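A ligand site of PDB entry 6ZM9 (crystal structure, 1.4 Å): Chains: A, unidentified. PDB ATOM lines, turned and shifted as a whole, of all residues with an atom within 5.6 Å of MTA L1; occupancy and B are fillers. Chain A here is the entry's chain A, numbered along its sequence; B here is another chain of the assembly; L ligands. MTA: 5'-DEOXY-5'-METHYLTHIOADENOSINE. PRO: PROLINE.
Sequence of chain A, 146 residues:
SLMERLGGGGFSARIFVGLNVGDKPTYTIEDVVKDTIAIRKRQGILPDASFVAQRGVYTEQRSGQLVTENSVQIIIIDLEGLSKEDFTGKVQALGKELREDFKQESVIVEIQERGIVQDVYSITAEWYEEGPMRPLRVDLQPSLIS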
ATOM      1  N   PHE A  16      -8.541   4.625  -4.223  1.00  0.00           N
ATOM      2  CA  PHE A  16      -8.103   3.254  -4.391  1.00  0.00           C
ATOM      3  C   PHE A  16      -7.405   3.110  -5.737  1.00  0.00           C
ATOM      4  O   PHE A  16      -8.035   3.361  -6.784  1.00  0.00           O
ATOM      5  CB  PHE A  16      -9.290   2.309  -4.304  1.00  0.00           C
ATOM      6  CG  PHE A  16      -9.965   2.308  -2.967  1.00  0.00           C
ATOM      7  CD1 PHE A  16     -10.954   3.227  -2.646  1.00  0.00           C
ATOM      8  CD2 PHE A  16      -9.603   1.369  -2.018  1.00  0.00           C
ATOM      9  CE1 PHE A  16     -11.585   3.199  -1.409  1.00  0.00           C
ATOM     10  CE2 PHE A  16     -10.247   1.317  -0.773  1.00  0.00           C
ATOM     11  CZ  PHE A  16     -11.228   2.220  -0.465  1.00  0.00           C
ATOM     12  N   VAL A  17      -6.139   2.677  -5.705  1.00  0.00           N
ATOM     13  CA  VAL A  17      -5.287   2.555  -6.894  1.00  0.00           C
ATOM     14  C   VAL A  17      -4.697   1.157  -6.924  1.00  0.00           C
ATOM     15  O   VAL A  17      -3.964   0.789  -5.993  1.00  0.00           O
ATOM     16  CB  VAL A  17      -4.130   3.578  -6.902  1.00  0.00           C
ATOM     17  CG1 VAL A  17      -3.400   3.526  -8.252  1.00  0.00           C
ATOM     18  CG2 VAL A  17      -4.591   4.992  -6.599  1.00  0.00           C
ATOM     19  N   GLY A  18      -4.950   0.406  -7.991  1.00  0.00           N
ATOM     20  CA  GLY A  18      -4.337  -0.888  -8.153  1.00  0.00           C
ATOM     21  C   GLY A  18      -2.921  -0.821  -8.708  1.00  0.00           C
ATOM     22  O   GLY A  18      -2.465   0.182  -9.273  1.00  0.00           O
ATOM     23  N   GLN A  54      -2.858  -3.061   0.356  1.00  0.00           N
ATOM     24  CA  GLN A  54      -4.027  -3.907   0.359  1.00  0.00           C
ATOM     25  C   GLN A  54      -3.848  -5.027  -0.658  1.00  0.00           C
ATOM     26  O   GLN A  54      -3.007  -4.935  -1.563  1.00  0.00           O
ATOM     27  CB  GLN A  54      -5.298  -3.184  -0.115  1.00  0.00           C
ATOM     28  CG  GLN A  54      -5.501  -1.853   0.497  1.00  0.00           C
ATOM     29  CD  GLN A  54      -6.837  -1.253   0.126  1.00  0.00           C
ATOM     30  OE1 GLN A  54      -7.600  -0.849   0.991  1.00  0.00           O
ATOM     31  NE2 GLN A  54      -7.083  -1.135  -1.169  1.00  0.00           N
ATOM     32  N   ARG A  55      -4.666  -6.054  -0.522  1.00  0.00           N
ATOM     33  CA  ARG A  55      -5.001  -6.948  -1.622  1.00  0.00           C
ATOM     34  C   ARG A  55      -6.345  -6.496  -2.164  1.00  0.00           C
ATOM     35  O   ARG A  55      -7.246  -6.150  -1.386  1.00  0.00           O
ATOM     36  CB  ARG A  55      -5.042  -8.406  -1.193  1.00  0.00           C
ATOM     37  CG  ARG A  55      -3.695  -8.919  -0.747  1.00  0.00           C
ATOM     38  CD  ARG A  55      -2.698  -9.066  -1.908  1.00  0.00           C
ATOM     39  NE  ARG A  55      -2.989 -10.245  -2.709  1.00  0.00           N
ATOM     40  CZ  ARG A  55      -2.494 -10.464  -3.929  1.00  0.00           C
ATOM     41  NH1 ARG A  55      -1.711  -9.580  -4.522  1.00  0.00           N
ATOM     42  NH2 ARG A  55      -2.808 -11.587  -4.555  1.00  0.00           N
ATOM     43  N   GLY A  56      -6.467  -6.441  -3.480  1.00  0.00           N
ATOM     44  CA  GLY A  56      -7.690  -5.968  -4.100  1.00  0.00           C
ATOM     45  C   GLY A  56      -8.189  -6.970  -5.125  1.00  0.00           C
ATOM     46  O   GLY A  56      -7.425  -7.691  -5.759  1.00  0.00           O
ATOM     47  N   VAL A  57      -9.510  -6.975  -5.283  1.00  0.00           N
ATOM     48  CA  VAL A  57     -10.190  -7.796  -6.266  1.00  0.00           C
ATOM     49  C   VAL A  57     -11.025  -6.858  -7.136  1.00  0.00           C
ATOM     50  O   VAL A  57     -11.780  -6.039  -6.600  1.00  0.00           O
ATOM     51  CB  VAL A  57     -11.074  -8.847  -5.582  1.00  0.00           C
ATOM     52  CG1 VAL A  57     -11.905  -9.632  -6.575  1.00  0.00           C
ATOM     53  CG2 VAL A  57     -10.214  -9.783  -4.739  1.00  0.00           C
ATOM     54  N   TYR A  58     -10.885  -6.986  -8.454  1.00  0.00           N
ATOM     55  CA  TYR A  58     -11.549  -6.128  -9.413  1.00  0.00           C
ATOM     56  C   TYR A  58     -11.967  -6.930 -10.638  1.00  0.00           C
ATOM     57  O   TYR A  58     -11.199  -7.733 -11.154  1.00  0.00           O
ATOM     58  CB  TYR A  58     -10.594  -5.038  -9.857  1.00  0.00           C
ATOM     59  CG  TYR A  58     -11.071  -4.137 -10.966  1.00  0.00           C
ATOM     60  CD1 TYR A  58     -11.964  -3.108 -10.708  1.00  0.00           C
ATOM     61  CD2 TYR A  58     -10.632  -4.298 -12.260  1.00  0.00           C
ATOM     62  CE1 TYR A  58     -12.391  -2.236 -11.713  1.00  0.00           C
ATOM     63  CE2 TYR A  58     -11.041  -3.440 -13.276  1.00  0.00           C
ATOM     64  CZ  TYR A  58     -11.944  -2.421 -12.992  1.00  0.00           C
ATOM     65  OH  TYR A  58     -12.362  -1.549 -13.982  1.00  0.00           O
ATOM     66  N   GLU A  69      -4.930  -8.407  -7.033  1.00  0.00           N
ATOM     67  CA  GLU A  69      -3.723  -7.613  -7.174  1.00  0.00           C
ATOM     68  C   GLU A  69      -3.355  -7.013  -5.821  1.00  0.00           C
ATOM     69  O   GLU A  69      -4.130  -7.011  -4.874  1.00  0.00           O
ATOM     70  CB  GLU A  69      -3.942  -6.461  -8.177  1.00  0.00           C
ATOM     71  CG  GLU A  69      -5.084  -5.507  -7.773  1.00  0.00           C
ATOM     72  CD  GLU A  69      -5.313  -4.345  -8.737  1.00  0.00           C
ATOM     73  OE1 GLU A  69      -4.532  -4.180  -9.713  1.00  0.00           O
ATOM     74  OE2 GLU A  69      -6.272  -3.586  -8.510  1.00  0.00           O
ATOM     75  N   ASN A  70      -2.140  -6.487  -5.755  1.00  0.00           N
ATOM     76  CA  ASN A  70      -1.823  -5.524  -4.710  1.00  0.00           C
ATOM     77  C   ASN A  70      -2.435  -4.181  -5.084  1.00  0.00           C
ATOM     78  O   ASN A  70      -2.522  -3.838  -6.270  1.00  0.00           O
ATOM     79  CB  ASN A  70      -0.314  -5.353  -4.567  1.00  0.00           C
ATOM     80  CG  ASN A  70       0.370  -6.590  -4.060  1.00  0.00           C
ATOM     81  OD1 ASN A  70      -0.214  -7.415  -3.349  1.00  0.00           O
ATOM     82  ND2 ASN A  70       1.645  -6.715  -4.393  1.00  0.00           N
ATOM     83  N   SER A  71      -2.873  -3.428  -4.085  1.00  0.00           N
ATOM     84  CA  SER A  71      -3.420  -2.106  -4.330  1.00  0.00           C
ATOM     85  C   SER A  71      -3.090  -1.194  -3.160  1.00  0.00           C
ATOM     86  O   SER A  71      -2.508  -1.618  -2.154  1.00  0.00           O
ATOM     87  CB  SER A  71      -4.926  -2.147  -4.614  1.00  0.00           C
ATOM     88  OG  SER A  71      -5.628  -2.607  -3.488  1.00  0.00           O
ATOM     89  N   GLN A 104      -4.036   2.506 -15.299  1.00  0.00           N
ATOM     90  CA  GLN A 104      -5.155   1.777 -14.713  1.00  0.00           C
ATOM     91  C   GLN A 104      -6.450   1.927 -15.503  1.00  0.00           C
ATOM     92  O   GLN A 104      -6.744   2.979 -16.074  1.00  0.00           O
ATOM     93  CB  GLN A 104      -5.402   2.263 -13.281  1.00  0.00           C
ATOM     94  CG  GLN A 104      -4.244   2.000 -12.358  1.00  0.00           C
ATOM     95  CD  GLN A 104      -4.056   0.527 -12.152  1.00  0.00           C
ATOM     96  OE1 GLN A 104      -4.908  -0.140 -11.569  1.00  0.00           O
ATOM     97  NE2 GLN A 104      -2.940  -0.009 -12.636  1.00  0.00           N
ATOM     98  N   SER A 106      -9.425   1.741 -13.915  1.00  0.00           N
ATOM     99  CA  SER A 106     -10.334   2.435 -13.008  1.00  0.00           C
ATOM    100  C   SER A 106      -9.603   2.810 -11.732  1.00  0.00           C
ATOM    101  O   SER A 106      -8.848   1.982 -11.208  1.00  0.00           O
ATOM    102  CB  SER A 106     -11.461   1.454 -12.621  1.00  0.00           C
ATOM    103  OG  SER A 106     -12.451   2.053 -11.808  1.00  0.00           O
ATOM    104  N   VAL A 107      -9.881   4.001 -11.211  1.00  0.00           N
ATOM    105  CA  VAL A 107      -9.475   4.450  -9.883  1.00  0.00           C
ATOM    106  C   VAL A 107     -10.749   4.895  -9.166  1.00  0.00           C
ATOM    107  O   VAL A 107     -11.562   5.614  -9.756  1.00  0.00           O
ATOM    108  CB  VAL A 107      -8.441   5.595  -9.951  1.00  0.00           C
ATOM    109  CG1 VAL A 107      -8.273   6.311  -8.634  1.00  0.00           C
ATOM    110  CG2 VAL A 107      -7.087   5.046 -10.408  1.00  0.00           C
ATOM    111  N   ILE A 108     -10.938   4.487  -7.919  1.00  0.00           N
ATOM    112  CA  ILE A 108     -12.117   4.885  -7.144  1.00  0.00           C
ATOM    113  C   ILE A 108     -11.741   6.017  -6.206  1.00  0.00           C
ATOM    114  O   ILE A 108     -10.731   5.934  -5.489  1.00  0.00           O
ATOM    115  CB  ILE A 108     -12.716   3.699  -6.362  1.00  0.00           C
ATOM    116  CG1 ILE A 108     -13.234   2.642  -7.329  1.00  0.00           C
ATOM    117  CG2 ILE A 108     -13.805   4.202  -5.424  1.00  0.00           C
ATOM    118  CD1 ILE A 108     -13.577   1.327  -6.652  1.00  0.00           C
ATOM    119  N   ASP B  48     -15.804  -7.728  -6.154  1.00  0.00           N
ATOM    120  CA  ASP B  48     -14.841  -6.642  -6.013  1.00  0.00           C
ATOM    121  C   ASP B  48     -14.826  -6.068  -4.599  1.00  0.00           C
ATOM    122  O   ASP B  48     -15.881  -5.791  -4.013  1.00  0.00           O
ATOM    123  CB  ASP B  48     -15.202  -5.537  -7.027  1.00  0.00           C
ATOM    124  CG  ASP B  48     -15.205  -6.011  -8.479  1.00  0.00           C
ATOM    125  OD1 ASP B  48     -15.429  -7.219  -8.743  1.00  0.00           O
ATOM    126  OD2 ASP B  48     -14.969  -5.142  -9.366  1.00  0.00           O
ATOM    127  N   ALA B  49     -13.620  -5.892  -4.063  1.00  0.00           N
ATOM    128  CA  ALA B  49     -13.442  -5.522  -2.662  1.00  0.00           C
ATOM    129  C   ALA B  49     -11.969  -5.239  -2.402  1.00  0.00           C
ATOM    130  O   ALA B  49     -11.111  -5.530  -3.247  1.00  0.00           O
ATOM    131  CB  ALA B  49     -13.906  -6.657  -1.743  1.00  0.00           C
ATOM    132  N   SER B  50     -11.686  -4.691  -1.228  1.00  0.00           N
ATOM    133  CA  SER B  50     -10.347  -4.448  -0.742  1.00  0.00           C
ATOM    134  C   SER B  50     -10.136  -5.222   0.553  1.00  0.00           C
ATOM    135  O   SER B  50     -11.075  -5.360   1.354  1.00  0.00           O
ATOM    136  CB  SER B  50     -10.108  -2.970  -0.463  1.00  0.00           C
ATOM    137  OG  SER B  50     -10.132  -2.232  -1.687  1.00  0.00           O
ATOM    138  N   PHE B  51      -8.913  -5.696   0.770  1.00  0.00           N
ATOM    139  CA  PHE B  51      -8.570  -6.516   1.933  1.00  0.00           C
ATOM    140  C   PHE B  51      -7.305  -5.924   2.560  1.00  0.00           C
ATOM    141  O   PHE B  51      -6.267  -5.846   1.908  1.00  0.00           O
ATOM    142  CB  PHE B  51      -8.320  -7.955   1.513  1.00  0.00           C
ATOM    143  CG  PHE B  51      -9.495  -8.621   0.825  1.00  0.00           C
ATOM    144  CD1 PHE B  51      -9.776  -8.371  -0.495  1.00  0.00           C
ATOM    145  CD2 PHE B  51     -10.321  -9.487   1.524  1.00  0.00           C
ATOM    146  CE1 PHE B  51     -10.843  -8.977  -1.119  1.00  0.00           C
ATOM    147  CE2 PHE B  51     -11.397 -10.097   0.898  1.00  0.00           C
ATOM    148  CZ  PHE B  51     -11.645  -9.849  -0.421  1.00  0.00           C
ATOM    149  N   ILE B  75     -13.128  -4.388   2.947  1.00  0.00           N
ATOM    150  CA  ILE B  75     -13.830  -3.144   2.632  1.00  0.00           C
ATOM    151  C   ILE B  75     -14.601  -3.374   1.335  1.00  0.00           C
ATOM    152  O   ILE B  75     -14.002  -3.685   0.306  1.00  0.00           O
ATOM    153  CB  ILE B  75     -12.861  -1.964   2.476  1.00  0.00           C
ATOM    154  CG1 ILE B  75     -12.035  -1.784   3.747  1.00  0.00           C
ATOM    155  CG2 ILE B  75     -13.611  -0.689   2.116  1.00  0.00           C
ATOM    156  CD1 ILE B  75     -10.853  -0.833   3.596  1.00  0.00           C
ATOM    157  N   ILE B  76     -15.925  -3.188   1.381  1.00  0.00           N
ATOM    158  CA  ILE B  76     -16.788  -3.431   0.239  1.00  0.00           C
ATOM    159  C   ILE B  76     -17.570  -2.156  -0.049  1.00  0.00           C
ATOM    160  O   ILE B  76     -18.347  -1.706   0.798  1.00  0.00           O
ATOM    161  CB  ILE B  76     -17.772  -4.581   0.504  1.00  0.00           C
ATOM    162  CG1 ILE B  76     -17.034  -5.902   0.683  1.00  0.00           C
ATOM    163  CG2 ILE B  76     -18.784  -4.679  -0.649  1.00  0.00           C
ATOM    164  CD1 ILE B  76     -17.899  -7.015   1.241  1.00  0.00           C
ATOM    165  N   ILE B  77     -17.364  -1.584  -1.237  1.00  0.00           N
ATOM    166  CA  ILE B  77     -18.205  -0.507  -1.733  1.00  0.00           C
ATOM    167  C   ILE B  77     -19.174  -1.116  -2.750  1.00  0.00           C
ATOM    168  O   ILE B  77     -18.739  -1.802  -3.680  1.00  0.00           O
ATOM    169  CB  ILE B  77     -17.351   0.604  -2.365  1.00  0.00           C
ATOM    170  CG1 ILE B  77     -16.357   1.175  -1.343  1.00  0.00           C
ATOM    171  CG2 ILE B  77     -18.287   1.681  -2.953  1.00  0.00           C
ATOM    172  CD1 ILE B  77     -15.356   2.076  -1.931  1.00  0.00           C
ATOM    173  N   ASP B  78     -20.479  -0.886  -2.567  1.00  0.00           N
ATOM    174  CA  ASP B  78     -21.453  -1.455  -3.500  1.00  0.00           C
ATOM    175  C   ASP B  78     -21.376  -0.669  -4.811  1.00  0.00           C
ATOM    176  O   ASP B  78     -21.672   0.531  -4.823  1.00  0.00           O
ATOM    177  CB  ASP B  78     -22.859  -1.358  -2.924  1.00  0.00           C
ATOM    178  CG  ASP B  78     -23.928  -1.868  -3.874  1.00  0.00           C
ATOM    179  OD1 ASP B  78     -23.592  -2.712  -4.739  1.00  0.00           O
ATOM    180  OD2 ASP B  78     -25.108  -1.432  -3.748  1.00  0.00           O
ATOM    181  N   LEU B  79     -20.991  -1.336  -5.898  1.00  0.00           N
ATOM    182  CA  LEU B  79     -20.972  -0.735  -7.223  1.00  0.00           C
ATOM    183  C   LEU B  79     -22.158  -1.164  -8.090  1.00  0.00           C
ATOM    184  O   LEU B  79     -22.227  -0.756  -9.258  1.00  0.00           O
ATOM    185  CB  LEU B  79     -19.663  -1.088  -7.967  1.00  0.00           C
ATOM    186  CG  LEU B  79     -18.368  -0.724  -7.253  1.00  0.00           C
ATOM    187  CD1 LEU B  79     -17.099  -1.011  -8.046  1.00  0.00           C
ATOM    188  CD2 LEU B  79     -18.343   0.743  -6.875  1.00  0.00           C
HETATM  189  CS  MTA L   1     -10.670   0.180  -8.906  1.00  0.00           C
HETATM  190  S5' MTA L   1      -9.598  -1.218  -8.999  1.00  0.00           S
HETATM  191  C5' MTA L   1      -8.329  -0.749  -7.818  1.00  0.00           C
HETATM  192  C4' MTA L   1      -8.550  -1.222  -6.393  1.00  0.00           C
HETATM  193  O4' MTA L   1      -9.796  -0.684  -5.905  1.00  0.00           O
HETATM  194  C2' MTA L   1      -9.382  -2.790  -4.820  1.00  0.00           C
HETATM  195  O2' MTA L   1      -8.408  -2.624  -3.811  1.00  0.00           O
HETATM  196  C3' MTA L   1      -8.660  -2.735  -6.171  1.00  0.00           C
HETATM  197  O3' MTA L   1      -7.404  -3.393  -6.163  1.00  0.00           O
HETATM  198  C1' MTA L   1     -10.294  -1.556  -4.903  1.00  0.00           C
HETATM  199  N9  MTA L   1     -11.676  -1.889  -5.224  1.00  0.00           N
HETATM  200  C8  MTA L   1     -12.250  -2.094  -6.457  1.00  0.00           C
HETATM  201  N7  MTA L   1     -13.542  -2.276  -6.426  1.00  0.00           N
HETATM  202  C5  MTA L   1     -13.859  -2.204  -5.078  1.00  0.00           C
HETATM  203  C6  MTA L   1     -15.082  -2.235  -4.383  1.00  0.00           C
HETATM  204  N6  MTA L   1     -16.278  -2.364  -4.965  1.00  0.00           N
HETATM  205  N1  MTA L   1     -15.033  -2.079  -3.029  1.00  0.00           N
HETATM  206  C2  MTA L   1     -13.847  -1.892  -2.446  1.00  0.00           C
HETATM  207  N3  MTA L   1     -12.639  -1.818  -2.992  1.00  0.00           N
HETATM  208  C4  MTA L   1     -12.710  -1.981  -4.326  1.00  0.00           C
HETATM  209  N   PRO L   2      -5.544  -2.747 -11.680  1.00  0.00           N
HETATM  210  CA  PRO L   2      -5.756  -3.519 -12.912  1.00  0.00           C
HETATM  211  C   PRO L   2      -5.802  -2.657 -14.162  1.00  0.00           C
HETATM  212  O   PRO L   2      -5.459  -3.119 -15.255  1.00  0.00           O
HETATM  213  CB  PRO L   2      -7.140  -4.134 -12.678  1.00  0.00           C
HETATM  214  CG  PRO L   2      -7.785  -3.184 -11.642  1.00  0.00           C
HETATM  215  CD  PRO L   2      -6.802  -2.172 -11.205  1.00  0.00           C
HETATM  216  OXT PRO L   2      -6.201  -1.496 -14.094  1.00  0.00           O
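The side-chain amide nitrogen of Gln 54 lies within hydrogen-bond range of the side-chain hydroxyl of Ser 50 of chain B, at 3.3 Å.
The side-chain amide oxygen (OE1) of Gln 104 lies close to the backbone carbonyl oxygen (O) of Gly 18, 3.4 Å away.
The backbone carbonyl oxygen of Ser 71 is in hydrogen-bond range of the backbone NH of Gln 54, at 2.9 Å.
The backbone carbonyl oxygen of Ala 49 of chain B is in hydrogen-bond range of the backbone NH of Val 57, at 3.0 Å.
O of Ile 108 lies within hydrogen-bond range of N of Phe 16, 2.8 Å away.
The backbone carbonyl oxygen (O) of Ser 50 of chain B sits at hydrogen-bond distance from the backbone NH (N) of Ile 75 of chain B, at 2.8 Å.
O of Glu 69 is in hydrogen-bond range of N of Gly 56, at 2.8 Å.
The side-chain amide oxygen (OE1) of Gln 104 is in hydrogen-bond range of a nitrogen (N) of PRO L2 (2.7 Å).
O2' of MTA L1 lies within hydrogen-bond range of NE2 of Gln 54, 3.3 Å away.
O of Ile 77 of chain B lies within hydrogen-bond range of N6 of MTA L1.
The side-chain carboxylate (OE2) of Glu 69 sits at hydrogen-bond distance from an oxygen (O3') of MTA L1 (2.6 Å).
N of PRO L2 lies within salt-bridge range of OE1 of Glu 69 (2.6 Å).
The side-chain hydroxyl (OG) of Ser 50 of chain B sits at hydrogen-bond distance from an oxygen (O2') of MTA L1, at 2.8 Å.
The side-chain hydroxyl (OG) of Ser 71 is in hydrogen-bond range of an oxygen (O2') of MTA L1 (2.8 Å).
N of Ile 77 of chain B sits at hydrogen-bond distance from N1 of MTA L1, 3.0 Å away.
Residues that only touch MTA L1: Phe 16 (3.4 Å), Gly 18 (3.6 Å), Gly 56 (3.3 Å), Val 57 (3.98 Å), Tyr 58 (3.5 Å), Ser 106 (3.4 Å), Ile 108 (3.6 Å), Asp 48 of chain B (3.6 Å), Ala 49 of chain B (3.5 Å), Ile 75 of chain B (3.3 Å), Ile 76 of chain B (3.9 Å) and Leu 79 of chain B (3.5 Å).
Hydrophobic or aromatic side chains that line MTA L1: Phe 16, Tyr 58, Ile 108, Ile 77 of chain B and Leu 79 of chain B.
Within 4 Å of MTA L1: Phe 16, Gly 18, Gln 54, Gly 56, Val 57, Tyr 58, Glu 69, Ser 71, Ser 106, Ile 108, Asp 48 of chain B, Ala 49 of chain B, Ser 50 of chain B, Ile 75 of chain B, Ile 76 of chain B, Ile 77 of chain B and Leu 79 of chain B.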
